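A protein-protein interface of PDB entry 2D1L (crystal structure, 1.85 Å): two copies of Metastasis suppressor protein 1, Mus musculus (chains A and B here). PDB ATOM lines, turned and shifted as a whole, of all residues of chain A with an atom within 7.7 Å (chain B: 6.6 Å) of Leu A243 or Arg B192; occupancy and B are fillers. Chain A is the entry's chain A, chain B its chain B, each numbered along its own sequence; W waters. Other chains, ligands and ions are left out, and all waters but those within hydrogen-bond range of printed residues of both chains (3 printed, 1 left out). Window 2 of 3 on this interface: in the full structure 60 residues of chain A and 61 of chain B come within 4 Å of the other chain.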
ATOM      1  N   GLY A  74      -5.872  -8.234 -12.301  1.00  0.00           N
ATOM      2  CA  GLY A  74      -5.350  -7.923 -13.630  1.00  0.00           C
ATOM      3  C   GLY A  74      -4.918  -9.134 -14.423  1.00  0.00           C
ATOM      4  O   GLY A  74      -4.977  -9.133 -15.659  1.00  0.00           O
ATOM      5  N   THR A  75      -4.482 -10.180 -13.727  1.00  0.00           N
ATOM      6  CA  THR A  75      -4.053 -11.391 -14.426  1.00  0.00           C
ATOM      7  C   THR A  75      -5.208 -12.016 -15.217  1.00  0.00           C
ATOM      8  O   THR A  75      -4.954 -12.635 -16.240  1.00  0.00           O
ATOM      9  CB  THR A  75      -3.439 -12.422 -13.465  1.00  0.00           C
ATOM     10  OG1 THR A  75      -2.535 -11.749 -12.588  1.00  0.00           O
ATOM     11  CG2 THR A  75      -2.670 -13.498 -14.226  1.00  0.00           C
ATOM     12  N   MET A 238       2.136  -3.760 -18.096  1.00  0.00           N
ATOM     13  CA  MET A 238       2.906  -2.647 -17.573  1.00  0.00           C
ATOM     14  C   MET A 238       3.323  -2.922 -16.130  1.00  0.00           C
ATOM     15  O   MET A 238       2.611  -3.606 -15.390  1.00  0.00           O
ATOM     16  CB  MET A 238       2.080  -1.362 -17.624  1.00  0.00           C
ATOM     17  CG  MET A 238       1.734  -0.888 -19.012  1.00  0.00           C
ATOM     18  SD  MET A 238       3.314  -0.661 -20.132  1.00  0.00           S
ATOM     19  CE  MET A 238       2.726   0.918 -21.182  1.00  0.00           C
ATOM     20  N   ASP A 239       4.488  -2.386 -15.761  1.00  0.00           N
ATOM     21  CA  ASP A 239       5.017  -2.450 -14.395  1.00  0.00           C
ATOM     22  C   ASP A 239       4.748  -3.765 -13.673  1.00  0.00           C
ATOM     23  O   ASP A 239       3.957  -3.797 -12.726  1.00  0.00           O
ATOM     24  CB  ASP A 239       4.479  -1.272 -13.589  1.00  0.00           C
ATOM     25  CG  ASP A 239       4.886   0.053 -14.188  1.00  0.00           C
ATOM     26  OD1 ASP A 239       6.064   0.177 -14.581  1.00  0.00           O
ATOM     27  OD2 ASP A 239       4.043   0.967 -14.272  1.00  0.00           O
ATOM     28  N   PRO A 240       5.413  -4.853 -14.116  1.00  0.00           N
ATOM     29  CA  PRO A 240       5.216  -6.194 -13.560  1.00  0.00           C
ATOM     30  C   PRO A 240       5.622  -6.316 -12.089  1.00  0.00           C
ATOM     31  O   PRO A 240       5.223  -7.273 -11.415  1.00  0.00           O
ATOM     32  CB  PRO A 240       6.109  -7.081 -14.440  1.00  0.00           C
ATOM     33  CG  PRO A 240       7.141  -6.143 -15.018  1.00  0.00           C
ATOM     34  CD  PRO A 240       6.410  -4.849 -15.209  1.00  0.00           C
ATOM     35  N   HIS A 241       6.375  -5.336 -11.597  1.00  0.00           N
ATOM     36  CA  HIS A 241       6.909  -5.354 -10.235  1.00  0.00           C
ATOM     37  C   HIS A 241       5.921  -4.761  -9.235  1.00  0.00           C
ATOM     38  O   HIS A 241       6.187  -4.692  -8.034  1.00  0.00           O
ATOM     39  CB  HIS A 241       8.194  -4.533 -10.203  1.00  0.00           C
ATOM     40  CG  HIS A 241       8.010  -3.124 -10.669  1.00  0.00           C
ATOM     41  ND1 HIS A 241       8.265  -2.033  -9.867  1.00  0.00           N
ATOM     42  CD2 HIS A 241       7.576  -2.628 -11.852  1.00  0.00           C
ATOM     43  CE1 HIS A 241       8.012  -0.925 -10.540  1.00  0.00           C
ATOM     44  NE2 HIS A 241       7.589  -1.260 -11.747  1.00  0.00           N
ATOM     45  N   LYS A 242       4.777  -4.331  -9.743  1.00  0.00           N
ATOM     46  CA  LYS A 242       3.836  -3.537  -8.969  1.00  0.00           C
ATOM     47  C   LYS A 242       2.438  -4.102  -9.175  1.00  0.00           C
ATOM     48  O   LYS A 242       2.175  -4.773 -10.178  1.00  0.00           O
ATOM     49  CB  LYS A 242       3.897  -2.096  -9.472  1.00  0.00           C
ATOM     50  CG  LYS A 242       3.435  -1.047  -8.510  1.00  0.00           C
ATOM     51  CD  LYS A 242       3.345   0.291  -9.215  1.00  0.00           C
ATOM     52  CE  LYS A 242       4.497   0.483 -10.183  1.00  0.00           C
ATOM     53  NZ  LYS A 242       4.742   1.932 -10.453  1.00  0.00           N
ATOM     54  N   LEU A 243       1.544  -3.831  -8.229  1.00  0.00           N
ATOM     55  CA  LEU A 243       0.145  -4.221  -8.376  1.00  0.00           C
ATOM     56  C   LEU A 243      -0.633  -3.202  -9.204  1.00  0.00           C
ATOM     57  O   LEU A 243      -0.702  -2.020  -8.837  1.00  0.00           O
ATOM     58  CB  LEU A 243      -0.528  -4.362  -7.005  1.00  0.00           C
ATOM     59  CG  LEU A 243      -0.441  -5.728  -6.330  1.00  0.00           C
ATOM     60  CD1 LEU A 243      -1.384  -5.776  -5.138  1.00  0.00           C
ATOM     61  CD2 LEU A 243      -0.750  -6.838  -7.330  1.00  0.00           C
ATOM     62  N   PRO A 244      -1.243  -3.656 -10.311  1.00  0.00           N
ATOM     63  CA  PRO A 244      -2.099  -2.754 -11.064  1.00  0.00           C
ATOM     64  C   PRO A 244      -3.358  -2.450 -10.247  1.00  0.00           C
ATOM     65  O   PRO A 244      -3.710  -3.211  -9.337  1.00  0.00           O
ATOM     66  CB  PRO A 244      -2.448  -3.561 -12.320  1.00  0.00           C
ATOM     67  CG  PRO A 244      -2.350  -4.992 -11.880  1.00  0.00           C
ATOM     68  CD  PRO A 244      -1.217  -5.013 -10.889  1.00  0.00           C
ATOM     69  N   SER A 245      -4.020  -1.340 -10.564  1.00  0.00           N
ATOM     70  CA  SER A 245      -5.240  -0.947  -9.865  1.00  0.00           C
ATOM     71  C   SER A 245      -6.297  -2.053  -9.910  1.00  0.00           C
ATOM     72  O   SER A 245      -7.076  -2.210  -8.972  1.00  0.00           O
ATOM     73  CB  SER A 245      -5.796   0.351 -10.455  1.00  0.00           C
ATOM     74  OG  SER A 245      -6.034   0.217 -11.846  1.00  0.00           O
ATOM     75  N   SER A 246      -6.303  -2.825 -10.996  1.00  0.00           N
ATOM     76  CA  SER A 246      -7.238  -3.940 -11.165  1.00  0.00           C
ATOM     77  C   SER A 246      -7.046  -5.071 -10.141  1.00  0.00           C
ATOM     78  O   SER A 246      -7.975  -5.834  -9.880  1.00  0.00           O
ATOM     79  CB  SER A 246      -7.124  -4.507 -12.582  1.00  0.00           C
ATOM     80  OG  SER A 246      -5.782  -4.868 -12.876  1.00  0.00           O
ATOM     81  N   SER A 247      -5.843  -5.177  -9.577  1.00  0.00           N
ATOM     82  CA  SER A 247      -5.536  -6.216  -8.585  1.00  0.00           C
ATOM     83  C   SER A 247      -5.667  -5.726  -7.138  1.00  0.00           C
ATOM     84  O   SER A 247      -5.330  -6.444  -6.193  1.00  0.00           O
ATOM     85  CB  SER A 247      -4.127  -6.768  -8.805  1.00  0.00           C
ATOM     86  OG  SER A 247      -4.016  -7.441 -10.045  1.00  0.00           O
ATOM     87  N   GLU A 248      -6.155  -4.506  -6.959  1.00  0.00           N
ATOM     88  CA  GLU A 248      -6.227  -3.935  -5.623  1.00  0.00           C
ATOM     89  C   GLU A 248      -7.635  -4.000  -5.041  1.00  0.00           C
ATOM     90  O   GLU A 248      -8.190  -2.994  -4.596  1.00  0.00           O
ATOM     91  CB  GLU A 248      -5.667  -2.514  -5.625  1.00  0.00           C
ATOM     92  CG  GLU A 248      -4.202  -2.471  -6.041  1.00  0.00           C
ATOM     93  CD  GLU A 248      -3.612  -1.082  -5.984  1.00  0.00           C
ATOM     94  OE1 GLU A 248      -4.383  -0.113  -5.818  1.00  0.00           O
ATOM     95  OE2 GLU A 248      -2.375  -0.959  -6.110  1.00  0.00           O
ATOM     96  N   GLN A 249      -8.199  -5.205  -5.052  1.00  0.00           N
ATOM     97  CA  GLN A 249      -9.504  -5.476  -4.458  1.00  0.00           C
ATOM     98  C   GLN A 249      -9.477  -6.776  -3.653  1.00  0.00           C
ATOM     99  O   GLN A 249      -8.775  -7.726  -4.006  1.00  0.00           O
ATOM    100  CB  GLN A 249     -10.578  -5.560  -5.540  1.00  0.00           C
ATOM    101  CG  GLN A 249     -10.911  -4.231  -6.192  1.00  0.00           C
ATOM    102  CD  GLN A 249     -11.907  -4.381  -7.322  1.00  0.00           C
ATOM    103  OE1 GLN A 249     -11.688  -5.153  -8.263  1.00  0.00           O
ATOM    104  NE2 GLN A 249     -13.011  -3.643  -7.238  1.00  0.00           N
ATOM    105  N   ILE B  22      -3.374 -18.692  -3.828  1.00  0.00           N
ATOM    106  CA  ILE B  22      -2.484 -18.185  -4.869  1.00  0.00           C
ATOM    107  C   ILE B  22      -1.275 -19.107  -5.014  1.00  0.00           C
ATOM    108  O   ILE B  22      -0.923 -19.525  -6.122  1.00  0.00           O
ATOM    109  CB  ILE B  22      -2.036 -16.743  -4.568  1.00  0.00           C
ATOM    110  CG1 ILE B  22      -3.247 -15.803  -4.501  1.00  0.00           C
ATOM    111  CG2 ILE B  22      -1.026 -16.245  -5.615  1.00  0.00           C
ATOM    112  CD1 ILE B  22      -2.879 -14.410  -3.986  1.00  0.00           C
ATOM    113  N   GLU B 187      -0.110 -10.898   6.654  1.00  0.00           N
ATOM    114  CA  GLU B 187      -0.830 -11.645   5.633  1.00  0.00           C
ATOM    115  C   GLU B 187      -1.225 -10.781   4.440  1.00  0.00           C
ATOM    116  O   GLU B 187      -1.202 -11.249   3.305  1.00  0.00           O
ATOM    117  CB  GLU B 187      -2.065 -12.327   6.235  1.00  0.00           C
ATOM    118  CG  GLU B 187      -1.733 -13.323   7.347  1.00  0.00           C
ATOM    119  CD  GLU B 187      -0.733 -14.384   6.904  1.00  0.00           C
ATOM    120  OE1 GLU B 187       0.408 -14.390   7.422  1.00  0.00           O
ATOM    121  OE2 GLU B 187      -1.083 -15.203   6.026  1.00  0.00           O
ATOM    122  N   LYS B 188      -1.583  -9.527   4.701  1.00  0.00           N
ATOM    123  CA  LYS B 188      -1.909  -8.570   3.646  1.00  0.00           C
ATOM    124  C   LYS B 188      -0.714  -8.366   2.707  1.00  0.00           C
ATOM    125  O   LYS B 188      -0.854  -8.363   1.475  1.00  0.00           O
ATOM    126  CB  LYS B 188      -2.320  -7.242   4.282  1.00  0.00           C
ATOM    127  CG  LYS B 188      -2.528  -6.089   3.317  1.00  0.00           C
ATOM    128  CD  LYS B 188      -2.224  -4.761   4.013  1.00  0.00           C
ATOM    129  CE  LYS B 188      -2.670  -3.558   3.188  1.00  0.00           C
ATOM    130  NZ  LYS B 188      -4.139  -3.317   3.306  1.00  0.00           N
ATOM    131  N   GLN B 189       0.460  -8.206   3.309  1.00  0.00           N
ATOM    132  CA  GLN B 189       1.701  -8.011   2.581  1.00  0.00           C
ATOM    133  C   GLN B 189       2.114  -9.273   1.839  1.00  0.00           C
ATOM    134  O   GLN B 189       2.583  -9.205   0.711  1.00  0.00           O
ATOM    135  CB  GLN B 189       2.801  -7.586   3.555  1.00  0.00           C
ATOM    136  CG  GLN B 189       2.517  -6.256   4.240  1.00  0.00           C
ATOM    137  CD  GLN B 189       3.429  -6.001   5.434  1.00  0.00           C
ATOM    138  OE1 GLN B 189       3.108  -5.199   6.324  1.00  0.00           O
ATOM    139  NE2 GLN B 189       4.575  -6.685   5.462  1.00  0.00           N
ATOM    140  N   ALA B 190       1.944 -10.429   2.471  1.00  0.00           N
ATOM    141  CA  ALA B 190       2.251 -11.696   1.820  1.00  0.00           C
ATOM    142  C   ALA B 190       1.354 -11.910   0.596  1.00  0.00           C
ATOM    143  O   ALA B 190       1.840 -12.308  -0.471  1.00  0.00           O
ATOM    144  CB  ALA B 190       2.111 -12.843   2.803  1.00  0.00           C
ATOM    145  N   VAL B 191       0.055 -11.633   0.735  1.00  0.00           N
ATOM    146  CA  VAL B 191      -0.859 -11.710  -0.409  1.00  0.00           C
ATOM    147  C   VAL B 191      -0.471 -10.706  -1.499  1.00  0.00           C
ATOM    148  O   VAL B 191      -0.466 -11.053  -2.667  1.00  0.00           O
ATOM    149  CB  VAL B 191      -2.360 -11.579   0.004  1.00  0.00           C
ATOM    150  CG1 VAL B 191      -3.264 -11.525  -1.221  1.00  0.00           C
ATOM    151  CG2 VAL B 191      -2.773 -12.755   0.897  1.00  0.00           C
ATOM    152  N   ARG B 192      -0.110  -9.475  -1.145  1.00  0.00           N
ATOM    153  CA  ARG B 192       0.368  -8.534  -2.152  1.00  0.00           C
ATOM    154  C   ARG B 192       1.561  -9.130  -2.911  1.00  0.00           C
ATOM    155  O   ARG B 192       1.625  -9.087  -4.148  1.00  0.00           O
ATOM    156  CB  ARG B 192       0.734  -7.200  -1.494  1.00  0.00           C
ATOM    157  CG  ARG B 192       1.543  -6.245  -2.374  1.00  0.00           C
ATOM    158  CD  ARG B 192       1.626  -4.863  -1.725  1.00  0.00           C
ATOM    159  NE  ARG B 192       0.298  -4.369  -1.366  1.00  0.00           N
ATOM    160  CZ  ARG B 192      -0.439  -3.569  -2.132  1.00  0.00           C
ATOM    161  NH1 ARG B 192      -1.639  -3.177  -1.720  1.00  0.00           N
ATOM    162  NH2 ARG B 192       0.028  -3.148  -3.304  1.00  0.00           N
ATOM    163  N   LYS B 193       2.502  -9.694  -2.165  1.00  0.00           N
ATOM    164  CA  LYS B 193       3.691 -10.275  -2.762  1.00  0.00           C
ATOM    165  C   LYS B 193       3.365 -11.431  -3.699  1.00  0.00           C
ATOM    166  O   LYS B 193       3.950 -11.514  -4.789  1.00  0.00           O
ATOM    167  CB  LYS B 193       4.659 -10.738  -1.674  1.00  0.00           C
ATOM    168  CG  LYS B 193       5.949 -11.314  -2.201  1.00  0.00           C
ATOM    169  CD  LYS B 193       7.022 -11.275  -1.130  1.00  0.00           C
ATOM    170  CE  LYS B 193       8.248 -12.065  -1.551  1.00  0.00           C
ATOM    171  NZ  LYS B 193       9.276 -12.087  -0.469  1.00  0.00           N
ATOM    172  N   ALA B 194       2.449 -12.314  -3.293  1.00  0.00           N
ATOM    173  CA  ALA B 194       2.034 -13.443  -4.158  1.00  0.00           C
ATOM    174  C   ALA B 194       1.294 -12.985  -5.419  1.00  0.00           C
ATOM    175  O   ALA B 194       1.539 -13.521  -6.503  1.00  0.00           O
ATOM    176  CB  ALA B 194       1.194 -14.493  -3.374  1.00  0.00           C
ATOM    177  N   LEU B 195       0.407 -11.993  -5.281  1.00  0.00           N
ATOM    178  CA  LEU B 195      -0.289 -11.389  -6.429  1.00  0.00           C
ATOM    179  C   LEU B 195       0.651 -10.769  -7.472  1.00  0.00           C
ATOM    180  O   LEU B 195       0.388 -10.840  -8.672  1.00  0.00           O
ATOM    181  CB  LEU B 195      -1.320 -10.348  -5.963  1.00  0.00           C
ATOM    182  CG  LEU B 195      -2.579 -10.877  -5.284  1.00  0.00           C
ATOM    183  CD1 LEU B 195      -3.439  -9.695  -4.761  1.00  0.00           C
ATOM    184  CD2 LEU B 195      -3.378 -11.791  -6.222  1.00  0.00           C
ATOM    185  N   ILE B 196       1.738 -10.162  -7.014  1.00  0.00           N
ATOM    186  CA  ILE B 196       2.719  -9.609  -7.919  1.00  0.00           C
ATOM    187  C   ILE B 196       3.485 -10.730  -8.634  1.00  0.00           C
ATOM    188  O   ILE B 196       3.713 -10.647  -9.837  1.00  0.00           O
ATOM    189  CB  ILE B 196       3.688  -8.647  -7.195  1.00  0.00           C
ATOM    190  CG1 ILE B 196       2.939  -7.383  -6.754  1.00  0.00           C
ATOM    191  CG2 ILE B 196       4.864  -8.282  -8.096  1.00  0.00           C
ATOM    192  CD1 ILE B 196       3.670  -6.570  -5.700  1.00  0.00           C
ATOM    193  N   GLU B 197       3.866 -11.774  -7.901  1.00  0.00           N
ATOM    194  CA  GLU B 197       4.591 -12.899  -8.504  1.00  0.00           C
ATOM    195  C   GLU B 197       3.711 -13.625  -9.527  1.00  0.00           C
ATOM    196  O   GLU B 197       4.174 -14.016 -10.592  1.00  0.00           O
ATOM    197  CB  GLU B 197       5.082 -13.877  -7.420  1.00  0.00           C
ATOM    198  CG  GLU B 197       5.910 -15.067  -7.947  1.00  0.00           C
ATOM    199  CD  GLU B 197       7.250 -14.659  -8.590  1.00  0.00           C
ATOM    200  OE1 GLU B 197       7.894 -13.699  -8.097  1.00  0.00           O
ATOM    201  OE2 GLU B 197       7.674 -15.322  -9.576  1.00  0.00           O
ATOM    202  N   ARG B 199       1.023 -12.440 -11.255  1.00  0.00           N
ATOM    203  CA  ARG B 199       0.873 -11.582 -12.421  1.00  0.00           C
ATOM    204  C   ARG B 199       2.194 -11.510 -13.155  1.00  0.00           C
ATOM    205  O   ARG B 199       2.214 -11.585 -14.378  1.00  0.00           O
ATOM    206  CB  ARG B 199       0.424 -10.172 -12.030  1.00  0.00           C
ATOM    207  CG  ARG B 199       0.235  -9.225 -13.240  1.00  0.00           C
ATOM    208  CD  ARG B 199      -0.495  -7.937 -12.869  1.00  0.00           C
ATOM    209  NE  ARG B 199      -0.498  -6.958 -13.957  1.00  0.00           N
ATOM    210  CZ  ARG B 199       0.466  -6.054 -14.181  1.00  0.00           C
ATOM    211  NH1 ARG B 199       1.550  -5.990 -13.403  1.00  0.00           N
ATOM    212  NH2 ARG B 199       0.353  -5.205 -15.196  1.00  0.00           N
HETATM  213  O   HOH W   1       1.286  -3.046 -12.011  1.00  0.00           O
HETATM  214  O   HOH W   2      -2.914  -6.720 -15.783  1.00  0.00           O
HETATM  215  O   HOH W   3      -0.694  -3.050 -17.200  1.00  0.00           O
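Water W1 lies within hydrogen-bond range of the backbone carbonyl oxygen (O) of Lys A242 (2.7 Å), the backbone carbonyl oxygen (O) of Asp A239 (2.9 Å) and the guanidinium group (NH1) of Arg B199 (3.3 Å). Water W2 lies within hydrogen-bond range of NE of Arg B199 and O of Gly A74. Water W3 bridges the backbone NH (N) of Met A238 (3.1 Å) and the guanidinium group (NH2) of Arg B199 (3.1 Å).
OG1 of Thr A75 touches CB of Arg B199, 3.4 Å away. CG2 of Ile B196 touches O of Pro A240, 3.5 Å away. Arg B199 touches Pro A240 (NH1 to CA, 3.7 Å). Ile B196 touches His A241 (CG2 to O, 3.8 Å). O of Lys A242 touches NH1 of Arg B199, at 3.5 Å. Arg B192 touches Leu A243. Leu A243 touches Leu B195. Ile B196 touches Leu A243. NE of Arg B199 touches CG of Pro A244, at 3.4 Å.
No position is printed for both chains. Of the 11 pairs that touch across the chains among the printed residues, none has its exchanged pair printed and touching as well.
O of Met A238 lies within hydrogen-bond range of NH2 of Arg B199 (2.8 Å). The guanidinium group (NH1) of Arg B199 lies within hydrogen-bond range of the backbone carbonyl oxygen (O) of Asp A239 (3.3 Å).
Printed residues of chain B within 4 Å of Pro A240: Ile B196 and Arg B199. Of the printed residues of chain B, Lys A242 touches Arg B199. Of the printed residues of chain B, Leu A243 touches Arg B192 (3.5 Å), Leu B195 (3.8 Å) and Ile B196 (3.8 Å). Printed residues of chain A within 4 Å of Arg B192: Leu A243. Printed residues of chain A within 4 Å of Leu B195: Leu A243 (3.8 Å). Glu B197 touches none of the printed residues of chain A. Printed residues of chain A within 4 Å of Arg B199: Thr A75 (3.4 Å), Met A238 (2.8 Å), Asp A239 (3.3 Å), Pro A240 (3.7 Å), Lys A242 (3.5 Å) and Pro A244 (3.4 Å). The nearest printed residue of chain B that does not touch Leu A243 is Arg B199 (5.5 Å). The nearest printed residue of chain B that does not touch His A241 is Arg B199 (5.2 Å).
Of the 13 printed residues of chain B, 4 touch a printed residue of chain A. Hydrophobic or aromatic side chains of chain B that line the printed part of chain A: Leu B195 and Ile B196. Among the printed residues, 11 pairs touch across the chains.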
